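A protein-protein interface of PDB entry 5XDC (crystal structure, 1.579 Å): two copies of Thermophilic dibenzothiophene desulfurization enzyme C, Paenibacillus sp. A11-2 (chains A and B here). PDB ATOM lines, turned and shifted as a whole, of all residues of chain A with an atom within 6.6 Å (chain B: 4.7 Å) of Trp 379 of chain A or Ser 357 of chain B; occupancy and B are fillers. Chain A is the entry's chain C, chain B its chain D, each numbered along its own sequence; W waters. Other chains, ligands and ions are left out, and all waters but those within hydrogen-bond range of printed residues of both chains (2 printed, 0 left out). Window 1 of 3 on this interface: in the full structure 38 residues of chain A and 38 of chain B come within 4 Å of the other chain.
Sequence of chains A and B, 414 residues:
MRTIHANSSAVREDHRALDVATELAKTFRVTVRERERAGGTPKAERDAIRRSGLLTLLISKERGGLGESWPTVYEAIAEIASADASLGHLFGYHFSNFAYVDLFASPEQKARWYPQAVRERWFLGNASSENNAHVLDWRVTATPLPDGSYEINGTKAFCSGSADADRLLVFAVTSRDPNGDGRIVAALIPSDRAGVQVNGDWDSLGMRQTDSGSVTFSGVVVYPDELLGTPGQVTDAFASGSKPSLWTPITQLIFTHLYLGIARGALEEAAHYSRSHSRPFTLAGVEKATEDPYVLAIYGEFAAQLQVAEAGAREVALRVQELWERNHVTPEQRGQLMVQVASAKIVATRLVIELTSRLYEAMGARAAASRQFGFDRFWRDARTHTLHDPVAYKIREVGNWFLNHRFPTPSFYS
Trp 379 of chain A touches four residues of chain B.
Printed residues of chain A within 4 Å of Ser 357 of chain B: Ile 353, Trp 379 and Arg 383.
Printed residues of chain A within 4 Å of Arg 358 of chain B: Arg 383.
Of the printed residues of chain B, Ile 353 of chain A touches Ser 357.
Printed residues of chain B within 4 Å of Arg 383 of chain A: Ser 357, Arg 358 and Tyr 360.
Of the printed residues of chain B, Asp 376 of chain A touches Trp 379.
Of the printed residues of chain B, Leu 205 of chain A touches Tyr 360 (3.7 Å) and Asp 376 (3.3 Å).
Phe 375 of chain A touches none of the printed residues of chain B.
The nearest printed residue of chain A that does not touch Arg 358 of chain B is Ile 353 of chain A (4.7 Å).
The side-chain hydroxyl (OG) of Ser 357 of chain A sits at hydrogen-bond distance from the indole nitrogen (NE1) of Trp 379 of chain B (3.0 Å).
The indole nitrogen (NE1) of Trp 379 of chain A sits at hydrogen-bond distance from the side-chain hydroxyl (OG) of Ser 357 of chain B (3.1 Å).
The guanidinium group of Arg 383 of chain A is in hydrogen-bond range of the backbone carbonyl oxygen of Ser 357 of chain B, at 3.0 Å.
Water W1 lies within hydrogen-bond range of the side-chain hydroxyl of Ser 357 of chain B and the backbone carbonyl oxygen of Ile 353 of chain A.
Water W2 bridges the side-chain hydroxyl (OG) of Ser 357 of chain A (2.7 Å) and the backbone carbonyl oxygen (O) of Ile 353 of chain B (2.8 Å).
O of Leu 205 of chain A sits at hydrogen-bond distance from NH1 of Arg 380 of chain A (3.0 Å).
The side-chain hydroxyl of Tyr 360 of chain A sits at hydrogen-bond distance from the backbone NH of Asp 376 of chain A.
OD2 of Asp 376 of chain A is in salt-bridge range of NE of Arg 380 of chain A.
The guanidinium group (NH1) of Arg 358 of chain B is in salt-bridge range of the side-chain carboxylate (OE2) of Glu 354 of chain B (3.1 Å).
The side-chain hydroxyl of Tyr 360 of chain B sits at hydrogen-bond distance from the backbone NH of Asp 376 of chain B, 3.1 Å away.
Ile 353 of chain A touches Ser 357 of chain B, and with the chains exchanged Ser 357 of chain A touches Ile 353 of chain B.
Tyr 360 of chain A touches Trp 379 of chain B, and with the chains exchanged Trp 379 of chain A touches Tyr 360 of chain B.
Asp 376 of chain A touches Trp 379 of chain B, and with the chains exchanged Trp 379 of chain A touches Asp 376 of chain B.
Trp 379 of chain B touches its own counterpart, Trp 379 of chain A.
Of the 14 pairs that touch across the chains among the printed residues, 9 have their exchanged pair printed and touching as well.
Hydrophobic or aromatic side chains of chain B within 4 Å of the printed part of chain A: Ile 353, Tyr 360 and Trp 379.
Along chain B the printed residues that touch a printed residue of chain A span positions 353 to 379.
Of the 20 printed residues of chain A, 7 touch a printed residue of chain B.
Printed residues of chain A that touch a printed residue of chain B: Leu 205, Ile 353, Ser 357, Tyr 360, Asp 376, Trp 379 and Arg 383.
Among the printed residues, 14 pairs touch across the chains.
Among the printed residues, pairs that only touch across the chains: Leu 205 of chain A with Tyr 360 of chain B, Leu 205 of chain A with Asp 376 of chain B, Ile 353 of chain A with Ser 357 of chain B, Ser 357 of chain A with Ile 353 of chain B, Tyr 360 of chain A with Trp 379 of chain B, Asp 376 of chain A with Trp 379 of chain B, Trp 379 of chain A with Tyr 360 of chain B, Trp 379 of chain A with Asp 376 of chain B, Trp 379 of chain A with Trp 379 of chain B, Arg 383 of chain A with Arg 358 of chain B and Arg 383 of chain A with Tyr 360 of chain B.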
ATOM      1  N   LEU A 205      18.686  -9.460  12.245  1.00  0.00           N
ATOM      2  CA  LEU A 205      18.318  -8.309  13.071  1.00  0.00           C
ATOM      3  C   LEU A 205      18.116  -7.063  12.221  1.00  0.00           C
ATOM      4  O   LEU A 205      17.077  -6.399  12.307  1.00  0.00           O
ATOM      5  CB  LEU A 205      19.391  -8.067  14.127  1.00  0.00           C
ATOM      6  CG  LEU A 205      19.217  -6.825  14.993  1.00  0.00           C
ATOM      7  CD1 LEU A 205      17.992  -6.942  15.886  1.00  0.00           C
ATOM      8  CD2 LEU A 205      20.467  -6.631  15.820  1.00  0.00           C
ATOM      9  N   GLY A 206      19.110  -6.730  11.393  1.00  0.00           N
ATOM     10  CA  GLY A 206      19.055  -5.625  10.460  1.00  0.00           C
ATOM     11  C   GLY A 206      19.591  -6.056   9.104  1.00  0.00           C
ATOM     12  O   GLY A 206      19.922  -7.231   8.935  1.00  0.00           O
ATOM     13  N   ILE A 262      23.906   5.457   6.942  1.00  0.00           N
ATOM     14  CA  ILE A 262      22.978   5.158   8.026  1.00  0.00           C
ATOM     15  C   ILE A 262      23.039   6.252   9.087  1.00  0.00           C
ATOM     16  O   ILE A 262      22.002   6.716   9.576  1.00  0.00           O
ATOM     17  CB  ILE A 262      23.283   3.770   8.613  1.00  0.00           C
ATOM     18  CG1 ILE A 262      22.993   2.672   7.586  1.00  0.00           C
ATOM     19  CG2 ILE A 262      22.471   3.515   9.877  1.00  0.00           C
ATOM     20  CD1 ILE A 262      23.662   1.361   7.942  1.00  0.00           C
ATOM     21  N   ALA A 266      19.829   8.481  10.070  1.00  0.00           N
ATOM     22  CA  ALA A 266      19.343   8.443  11.447  1.00  0.00           C
ATOM     23  C   ALA A 266      19.303   9.838  12.056  1.00  0.00           C
ATOM     24  O   ALA A 266      18.311  10.227  12.692  1.00  0.00           O
ATOM     25  CB  ALA A 266      20.229   7.510  12.279  1.00  0.00           C
ATOM     26  N   VAL A 352      28.313   5.553  14.078  1.00  0.00           N
ATOM     27  CA  VAL A 352      26.960   5.107  13.757  1.00  0.00           C
ATOM     28  C   VAL A 352      26.379   4.285  14.902  1.00  0.00           C
ATOM     29  O   VAL A 352      25.192   4.404  15.222  1.00  0.00           O
ATOM     30  CB  VAL A 352      26.930   4.340  12.422  1.00  0.00           C
ATOM     31  CG1 VAL A 352      27.619   2.980  12.520  1.00  0.00           C
ATOM     32  CG2 VAL A 352      25.477   4.211  11.954  1.00  0.00           C
ATOM     33  N   ILE A 353      27.196   3.463  15.551  1.00  0.00           N
ATOM     34  CA  ILE A 353      26.684   2.640  16.645  1.00  0.00           C
ATOM     35  C   ILE A 353      26.264   3.508  17.836  1.00  0.00           C
ATOM     36  O   ILE A 353      25.225   3.266  18.458  1.00  0.00           O
ATOM     37  CB  ILE A 353      27.731   1.584  17.040  1.00  0.00           C
ATOM     38  CG1 ILE A 353      27.928   0.571  15.903  1.00  0.00           C
ATOM     39  CG2 ILE A 353      27.340   0.861  18.316  1.00  0.00           C
ATOM     40  CD1 ILE A 353      26.658  -0.219  15.496  1.00  0.00           C
ATOM     41  N   GLU A 354      27.052   4.527  18.174  1.00  0.00           N
ATOM     42  CA  GLU A 354      26.645   5.405  19.267  1.00  0.00           C
ATOM     43  C   GLU A 354      25.415   6.210  18.881  1.00  0.00           C
ATOM     44  O   GLU A 354      24.416   6.232  19.608  1.00  0.00           O
ATOM     45  CB  GLU A 354      27.778   6.352  19.668  1.00  0.00           C
ATOM     46  CG  GLU A 354      27.390   7.150  20.918  1.00  0.00           C
ATOM     47  CD  GLU A 354      28.499   7.995  21.503  1.00  0.00           C
ATOM     48  OE1 GLU A 354      28.352   8.393  22.686  1.00  0.00           O
ATOM     49  OE2 GLU A 354      29.493   8.268  20.789  1.00  0.00           O
ATOM     50  N   THR A 356      23.008   5.952  16.631  1.00  0.00           N
ATOM     51  CA  THR A 356      21.706   5.344  16.400  1.00  0.00           C
ATOM     52  C   THR A 356      21.031   4.916  17.698  1.00  0.00           C
ATOM     53  O   THR A 356      19.803   4.781  17.732  1.00  0.00           O
ATOM     54  CB  THR A 356      21.832   4.148  15.447  1.00  0.00           C
ATOM     55  OG1 THR A 356      22.759   3.191  15.958  1.00  0.00           O
ATOM     56  CG2 THR A 356      22.291   4.612  14.066  1.00  0.00           C
ATOM     57  N   SER A 357      21.803   4.701  18.757  1.00  0.00           N
ATOM     58  CA  SER A 357      21.250   4.402  20.069  1.00  0.00           C
ATOM     59  C   SER A 357      20.992   5.670  20.883  1.00  0.00           C
ATOM     60  O   SER A 357      19.910   5.829  21.446  1.00  0.00           O
ATOM     61  CB  SER A 357      22.201   3.457  20.819  1.00  0.00           C
ATOM     62  OG  SER A 357      21.765   3.255  22.145  1.00  0.00           O
ATOM     63  N   TYR A 360      17.898   8.570  20.788  1.00  0.00           N
ATOM     64  CA  TYR A 360      16.659   8.458  21.551  1.00  0.00           C
ATOM     65  C   TYR A 360      16.645   9.429  22.713  1.00  0.00           C
ATOM     66  O   TYR A 360      15.587   9.956  23.072  1.00  0.00           O
ATOM     67  CB  TYR A 360      16.465   7.041  22.079  1.00  0.00           C
ATOM     68  CG  TYR A 360      15.882   6.065  21.072  1.00  0.00           C
ATOM     69  CD1 TYR A 360      14.517   5.979  20.879  1.00  0.00           C
ATOM     70  CD2 TYR A 360      16.703   5.246  20.312  1.00  0.00           C
ATOM     71  CE1 TYR A 360      13.970   5.087  19.969  1.00  0.00           C
ATOM     72  CE2 TYR A 360      16.164   4.347  19.389  1.00  0.00           C
ATOM     73  CZ  TYR A 360      14.796   4.278  19.232  1.00  0.00           C
ATOM     74  OH  TYR A 360      14.230   3.413  18.333  1.00  0.00           O
ATOM     75  N   PHE A 375      12.313   3.822  14.473  1.00  0.00           N
ATOM     76  CA  PHE A 375      13.638   4.433  14.426  1.00  0.00           C
ATOM     77  C   PHE A 375      14.742   3.423  14.709  1.00  0.00           C
ATOM     78  O   PHE A 375      15.889   3.636  14.290  1.00  0.00           O
ATOM     79  CB  PHE A 375      13.719   5.589  15.421  1.00  0.00           C
ATOM     80  CG  PHE A 375      15.007   6.368  15.351  1.00  0.00           C
ATOM     81  CD1 PHE A 375      15.198   7.369  14.405  1.00  0.00           C
ATOM     82  CD2 PHE A 375      16.046   6.083  16.233  1.00  0.00           C
ATOM     83  CE1 PHE A 375      16.393   8.077  14.345  1.00  0.00           C
ATOM     84  CE2 PHE A 375      17.234   6.795  16.175  1.00  0.00           C
ATOM     85  CZ  PHE A 375      17.402   7.789  15.232  1.00  0.00           C
ATOM     86  N   ASP A 376      14.427   2.332  15.412  1.00  0.00           N
ATOM     87  CA  ASP A 376      15.434   1.347  15.759  1.00  0.00           C
ATOM     88  C   ASP A 376      16.007   0.640  14.536  1.00  0.00           C
ATOM     89  O   ASP A 376      17.008  -0.068  14.668  1.00  0.00           O
ATOM     90  CB  ASP A 376      14.833   0.321  16.704  1.00  0.00           C
ATOM     91  CG  ASP A 376      13.665  -0.421  16.089  1.00  0.00           C
ATOM     92  OD1 ASP A 376      12.665   0.251  15.750  1.00  0.00           O
ATOM     93  OD2 ASP A 376      13.756  -1.665  15.966  1.00  0.00           O
ATOM     94  N   ARG A 377      15.363   0.771  13.374  1.00  0.00           N
ATOM     95  CA  ARG A 377      15.908   0.228  12.132  1.00  0.00           C
ATOM     96  C   ARG A 377      17.347   0.679  11.905  1.00  0.00           C
ATOM     97  O   ARG A 377      18.189  -0.115  11.474  1.00  0.00           O
ATOM     98  CB  ARG A 377      15.011   0.641  10.964  1.00  0.00           C
ATOM     99  CG  ARG A 377      15.500   0.215   9.589  1.00  0.00           C
ATOM    100  CD  ARG A 377      14.458   0.544   8.499  1.00  0.00           C
ATOM    101  NE  ARG A 377      14.120   1.954   8.468  1.00  0.00           N
ATOM    102  CZ  ARG A 377      14.796   2.888   7.818  1.00  0.00           C
ATOM    103  NH1 ARG A 377      15.872   2.573   7.110  1.00  0.00           N
ATOM    104  NH2 ARG A 377      14.397   4.151   7.896  1.00  0.00           N
ATOM    105  N   PHE A 378      17.651   1.951  12.184  1.00  0.00           N
ATOM    106  CA  PHE A 378      19.001   2.450  11.930  1.00  0.00           C
ATOM    107  C   PHE A 378      20.022   1.718  12.796  1.00  0.00           C
ATOM    108  O   PHE A 378      21.043   1.239  12.290  1.00  0.00           O
ATOM    109  CB  PHE A 378      19.087   3.961  12.161  1.00  0.00           C
ATOM    110  CG  PHE A 378      18.207   4.778  11.252  1.00  0.00           C
ATOM    111  CD1 PHE A 378      18.588   5.045   9.946  1.00  0.00           C
ATOM    112  CD2 PHE A 378      17.005   5.289  11.710  1.00  0.00           C
ATOM    113  CE1 PHE A 378      17.783   5.796   9.116  1.00  0.00           C
ATOM    114  CE2 PHE A 378      16.192   6.032  10.889  1.00  0.00           C
ATOM    115  CZ  PHE A 378      16.590   6.301   9.587  1.00  0.00           C
ATOM    116  N   TRP A 379      19.755   1.598  14.101  1.00  0.00           N
ATOM    117  CA  TRP A 379      20.652   0.824  14.957  1.00  0.00           C
ATOM    118  C   TRP A 379      20.713  -0.632  14.512  1.00  0.00           C
ATOM    119  O   TRP A 379      21.800  -1.208  14.429  1.00  0.00           O
ATOM    120  CB  TRP A 379      20.228   0.919  16.426  1.00  0.00           C
ATOM    121  CG  TRP A 379      21.043   0.062  17.331  1.00  0.00           C
ATOM    122  CD1 TRP A 379      22.249   0.370  17.905  1.00  0.00           C
ATOM    123  CD2 TRP A 379      20.709  -1.247  17.789  1.00  0.00           C
ATOM    124  NE1 TRP A 379      22.685  -0.671  18.686  1.00  0.00           N
ATOM    125  CE2 TRP A 379      21.761  -1.679  18.640  1.00  0.00           C
ATOM    126  CE3 TRP A 379      19.619  -2.090  17.583  1.00  0.00           C
ATOM    127  CZ2 TRP A 379      21.754  -2.921  19.263  1.00  0.00           C
ATOM    128  CZ3 TRP A 379      19.622  -3.327  18.194  1.00  0.00           C
ATOM    129  CH2 TRP A 379      20.675  -3.731  19.025  1.00  0.00           C
ATOM    130  N   ARG A 380      19.563  -1.243  14.201  1.00  0.00           N
ATOM    131  CA  ARG A 380      19.576  -2.651  13.817  1.00  0.00           C
ATOM    132  C   ARG A 380      20.437  -2.877  12.577  1.00  0.00           C
ATOM    133  O   ARG A 380      21.238  -3.823  12.533  1.00  0.00           O
ATOM    134  CB  ARG A 380      18.152  -3.160  13.581  1.00  0.00           C
ATOM    135  CG  ARG A 380      17.382  -3.385  14.861  1.00  0.00           C
ATOM    136  CD  ARG A 380      16.042  -4.073  14.645  1.00  0.00           C
ATOM    137  NE  ARG A 380      15.035  -3.210  14.032  1.00  0.00           N
ATOM    138  CZ  ARG A 380      14.669  -3.249  12.753  1.00  0.00           C
ATOM    139  NH1 ARG A 380      15.235  -4.109  11.915  1.00  0.00           N
ATOM    140  NH2 ARG A 380      13.722  -2.434  12.308  1.00  0.00           N
ATOM    141  N   ASP A 381      20.280  -2.021  11.565  1.00  0.00           N
ATOM    142  CA  ASP A 381      21.050  -2.170  10.328  1.00  0.00           C
ATOM    143  C   ASP A 381      22.538  -1.973  10.585  1.00  0.00           C
ATOM    144  O   ASP A 381      23.374  -2.759  10.125  1.00  0.00           O
ATOM    145  CB  ASP A 381      20.574  -1.170   9.276  1.00  0.00           C
ATOM    146  CG  ASP A 381      19.186  -1.455   8.778  1.00  0.00           C
ATOM    147  OD1 ASP A 381      18.750  -2.631   8.842  1.00  0.00           O
ATOM    148  OD2 ASP A 381      18.546  -0.497   8.325  1.00  0.00           O
ATOM    149  N   ALA A 382      22.889  -0.910  11.301  1.00  0.00           N
ATOM    150  CA  ALA A 382      24.295  -0.638  11.574  1.00  0.00           C
ATOM    151  C   ALA A 382      24.895  -1.688  12.503  1.00  0.00           C
ATOM    152  O   ALA A 382      26.006  -2.169  12.265  1.00  0.00           O
ATOM    153  CB  ALA A 382      24.442   0.757  12.163  1.00  0.00           C
ATOM    154  N   ARG A 383      24.169  -2.081  13.559  1.00  0.00           N
ATOM    155  CA  ARG A 383      24.714  -3.065  14.491  1.00  0.00           C
ATOM    156  C   ARG A 383      24.988  -4.391  13.787  1.00  0.00           C
ATOM    157  O   ARG A 383      25.948  -5.094  14.133  1.00  0.00           O
ATOM    158  CB  ARG A 383      23.747  -3.279  15.662  1.00  0.00           C
ATOM    159  CG  ARG A 383      24.181  -4.300  16.716  1.00  0.00           C
ATOM    160  CD  ARG A 383      25.363  -3.823  17.513  1.00  0.00           C
ATOM    161  NE  ARG A 383      26.595  -3.851  16.726  1.00  0.00           N
ATOM    162  CZ  ARG A 383      27.788  -3.449  17.156  1.00  0.00           C
ATOM    163  NH1 ARG A 383      27.969  -3.037  18.407  1.00  0.00           N
ATOM    164  NH2 ARG A 383      28.819  -3.472  16.328  1.00  0.00           N
ATOM    165  N   THR A 384      24.155  -4.740  12.804  1.00  0.00           N
ATOM    166  CA  THR A 384      24.337  -5.980  12.047  1.00  0.00           C
ATOM    167  C   THR A 384      25.578  -5.917  11.168  1.00  0.00           C
ATOM    168  O   THR A 384      26.486  -6.740  11.311  1.00  0.00           O
ATOM    169  CB  THR A 384      23.079  -6.286  11.215  1.00  0.00           C
ATOM    170  OG1 THR A 384      21.972  -6.501  12.093  1.00  0.00           O
ATOM    171  CG2 THR A 384      23.238  -7.541  10.390  1.00  0.00           C
ATOM    172  N   ILE B 353      22.956   1.054  28.517  1.00  0.00           N
ATOM    173  CA  ILE B 353      22.771   1.459  27.125  1.00  0.00           C
ATOM    174  C   ILE B 353      24.005   1.117  26.302  1.00  0.00           C
ATOM    175  O   ILE B 353      23.890   0.665  25.155  1.00  0.00           O
ATOM    176  CB  ILE B 353      22.422   2.956  27.028  1.00  0.00           C
ATOM    177  CG1 ILE B 353      21.047   3.232  27.637  1.00  0.00           C
ATOM    178  CG2 ILE B 353      22.446   3.441  25.598  1.00  0.00           C
ATOM    179  CD1 ILE B 353      19.885   2.452  26.994  1.00  0.00           C
ATOM    180  N   GLU B 354      25.202   1.293  26.872  1.00  0.00           N
ATOM    181  CA  GLU B 354      26.423   0.986  26.130  1.00  0.00           C
ATOM    182  C   GLU B 354      26.627  -0.520  26.011  1.00  0.00           C
ATOM    183  O   GLU B 354      26.962  -1.023  24.934  1.00  0.00           O
ATOM    184  CB  GLU B 354      27.630   1.648  26.805  1.00  0.00           C
ATOM    185  CG  GLU B 354      28.974   1.439  26.088  1.00  0.00           C
ATOM    186  CD  GLU B 354      29.155   2.288  24.833  1.00  0.00           C
ATOM    187  OE1 GLU B 354      28.225   3.024  24.448  1.00  0.00           O
ATOM    188  OE2 GLU B 354      30.251   2.216  24.233  1.00  0.00           O
ATOM    189  N   LEU B 355      26.399  -1.254  27.103  1.00  0.00           N
ATOM    190  CA  LEU B 355      26.676  -2.679  27.143  1.00  0.00           C
ATOM    191  C   LEU B 355      25.759  -3.464  26.209  1.00  0.00           C
ATOM    192  O   LEU B 355      26.215  -4.366  25.492  1.00  0.00           O
ATOM    193  CB  LEU B 355      26.534  -3.128  28.601  1.00  0.00           C
ATOM    194  CG  LEU B 355      26.631  -4.537  29.116  1.00  0.00           C
ATOM    195  CD1 LEU B 355      26.778  -4.397  30.633  1.00  0.00           C
ATOM    196  CD2 LEU B 355      25.376  -5.303  28.777  1.00  0.00           C
ATOM    197  N   THR B 356      24.467  -3.147  26.205  1.00  0.00           N
ATOM    198  CA  THR B 356      23.524  -3.942  25.428  1.00  0.00           C
ATOM    199  C   THR B 356      23.746  -3.779  23.932  1.00  0.00           C
ATOM    200  O   THR B 356      23.371  -4.670  23.168  1.00  0.00           O
ATOM    201  CB  THR B 356      22.076  -3.593  25.792  1.00  0.00           C
ATOM    202  OG1 THR B 356      21.828  -2.197  25.582  1.00  0.00           O
ATOM    203  CG2 THR B 356      21.783  -3.955  27.230  1.00  0.00           C
ATOM    204  N   SER B 357      24.376  -2.690  23.501  1.00  0.00           N
ATOM    205  CA  SER B 357      24.758  -2.507  22.104  1.00  0.00           C
ATOM    206  C   SER B 357      26.152  -3.065  21.804  1.00  0.00           C
ATOM    207  O   SER B 357      26.338  -3.790  20.817  1.00  0.00           O
ATOM    208  CB  SER B 357      24.681  -1.012  21.761  1.00  0.00           C
ATOM    209  OG  SER B 357      25.165  -0.745  20.468  1.00  0.00           O
ATOM    210  N   ARG B 358      27.145  -2.758  22.650  1.00  0.00           N
ATOM    211  CA  ARG B 358      28.533  -3.086  22.333  1.00  0.00           C
ATOM    212  C   ARG B 358      28.855  -4.563  22.499  1.00  0.00           C
ATOM    213  O   ARG B 358      29.849  -5.030  21.938  1.00  0.00           O
ATOM    214  CB  ARG B 358      29.495  -2.302  23.217  1.00  0.00           C
ATOM    215  CG  ARG B 358      29.382  -0.804  23.127  1.00  0.00           C
ATOM    216  CD  ARG B 358      30.160  -0.204  21.977  1.00  0.00           C
ATOM    217  NE  ARG B 358      31.479  -0.807  21.783  1.00  0.00           N
ATOM    218  CZ  ARG B 358      32.494  -0.714  22.636  1.00  0.00           C
ATOM    219  NH1 ARG B 358      32.358  -0.052  23.783  1.00  0.00           N
ATOM    220  NH2 ARG B 358      33.649  -1.307  22.346  1.00  0.00           N
ATOM    221  N   LEU B 359      28.084  -5.306  23.285  1.00  0.00           N
ATOM    222  CA  LEU B 359      28.437  -6.705  23.486  1.00  0.00           C
ATOM    223  C   LEU B 359      28.358  -7.509  22.197  1.00  0.00           C
ATOM    224  O   LEU B 359      28.997  -8.560  22.104  1.00  0.00           O
ATOM    225  CB  LEU B 359      27.546  -7.328  24.555  1.00  0.00           C
ATOM    226  CG  LEU B 359      28.056  -7.154  25.979  1.00  0.00           C
ATOM    227  CD1 LEU B 359      26.935  -7.531  26.959  1.00  0.00           C
ATOM    228  CD2 LEU B 359      29.261  -8.009  26.170  1.00  0.00           C
ATOM    229  N   TYR B 360      27.602  -7.047  21.204  1.00  0.00           N
ATOM    230  CA  TYR B 360      27.643  -7.706  19.901  1.00  0.00           C
ATOM    231  C   TYR B 360      29.065  -7.808  19.376  1.00  0.00           C
ATOM    232  O   TYR B 360      29.405  -8.773  18.679  1.00  0.00           O
ATOM    233  CB  TYR B 360      26.788  -6.951  18.891  1.00  0.00           C
ATOM    234  CG  TYR B 360      25.312  -7.271  18.967  1.00  0.00           C
ATOM    235  CD1 TYR B 360      24.796  -8.366  18.298  1.00  0.00           C
ATOM    236  CD2 TYR B 360      24.437  -6.472  19.687  1.00  0.00           C
ATOM    237  CE1 TYR B 360      23.462  -8.659  18.345  1.00  0.00           C
ATOM    238  CE2 TYR B 360      23.087  -6.751  19.724  1.00  0.00           C
ATOM    239  CZ  TYR B 360      22.614  -7.856  19.061  1.00  0.00           C
ATOM    240  OH  TYR B 360      21.289  -8.176  19.087  1.00  0.00           O
ATOM    241  N   ASP B 376      18.844  -8.562  20.914  1.00  0.00           N
ATOM    242  CA  ASP B 376      18.502  -7.148  20.854  1.00  0.00           C
ATOM    243  C   ASP B 376      17.413  -6.776  21.851  1.00  0.00           C
ATOM    244  O   ASP B 376      17.212  -5.588  22.116  1.00  0.00           O
ATOM    245  CB  ASP B 376      18.075  -6.762  19.428  1.00  0.00           C
ATOM    246  CG  ASP B 376      16.856  -7.525  18.960  1.00  0.00           C
ATOM    247  OD1 ASP B 376      16.946  -8.769  18.885  1.00  0.00           O
ATOM    248  OD2 ASP B 376      15.813  -6.884  18.708  1.00  0.00           O
ATOM    249  N   TRP B 379      18.802  -4.447  24.627  1.00  0.00           N
ATOM    250  CA  TRP B 379      18.919  -3.043  24.238  1.00  0.00           C
ATOM    251  C   TRP B 379      17.543  -2.402  24.079  1.00  0.00           C
ATOM    252  O   TRP B 379      17.313  -1.274  24.529  1.00  0.00           O
ATOM    253  CB  TRP B 379      19.726  -2.913  22.943  1.00  0.00           C
ATOM    254  CG  TRP B 379      19.770  -1.515  22.428  1.00  0.00           C
ATOM    255  CD1 TRP B 379      20.625  -0.522  22.810  1.00  0.00           C
ATOM    256  CD2 TRP B 379      18.922  -0.947  21.420  1.00  0.00           C
ATOM    257  NE1 TRP B 379      20.346   0.634  22.122  1.00  0.00           N
ATOM    258  CE2 TRP B 379      19.311   0.397  21.254  1.00  0.00           C
ATOM    259  CE3 TRP B 379      17.866  -1.444  20.651  1.00  0.00           C
ATOM    260  CZ2 TRP B 379      18.691   1.247  20.344  1.00  0.00           C
ATOM    261  CZ3 TRP B 379      17.235  -0.599  19.758  1.00  0.00           C
ATOM    262  CH2 TRP B 379      17.659   0.741  19.605  1.00  0.00           C
HETATM  263  O   HOH W   1      25.535   1.917  20.875  1.00  0.00           O
HETATM  264  O   HOH W   2      24.214   2.448  23.028  1.00  0.00           O
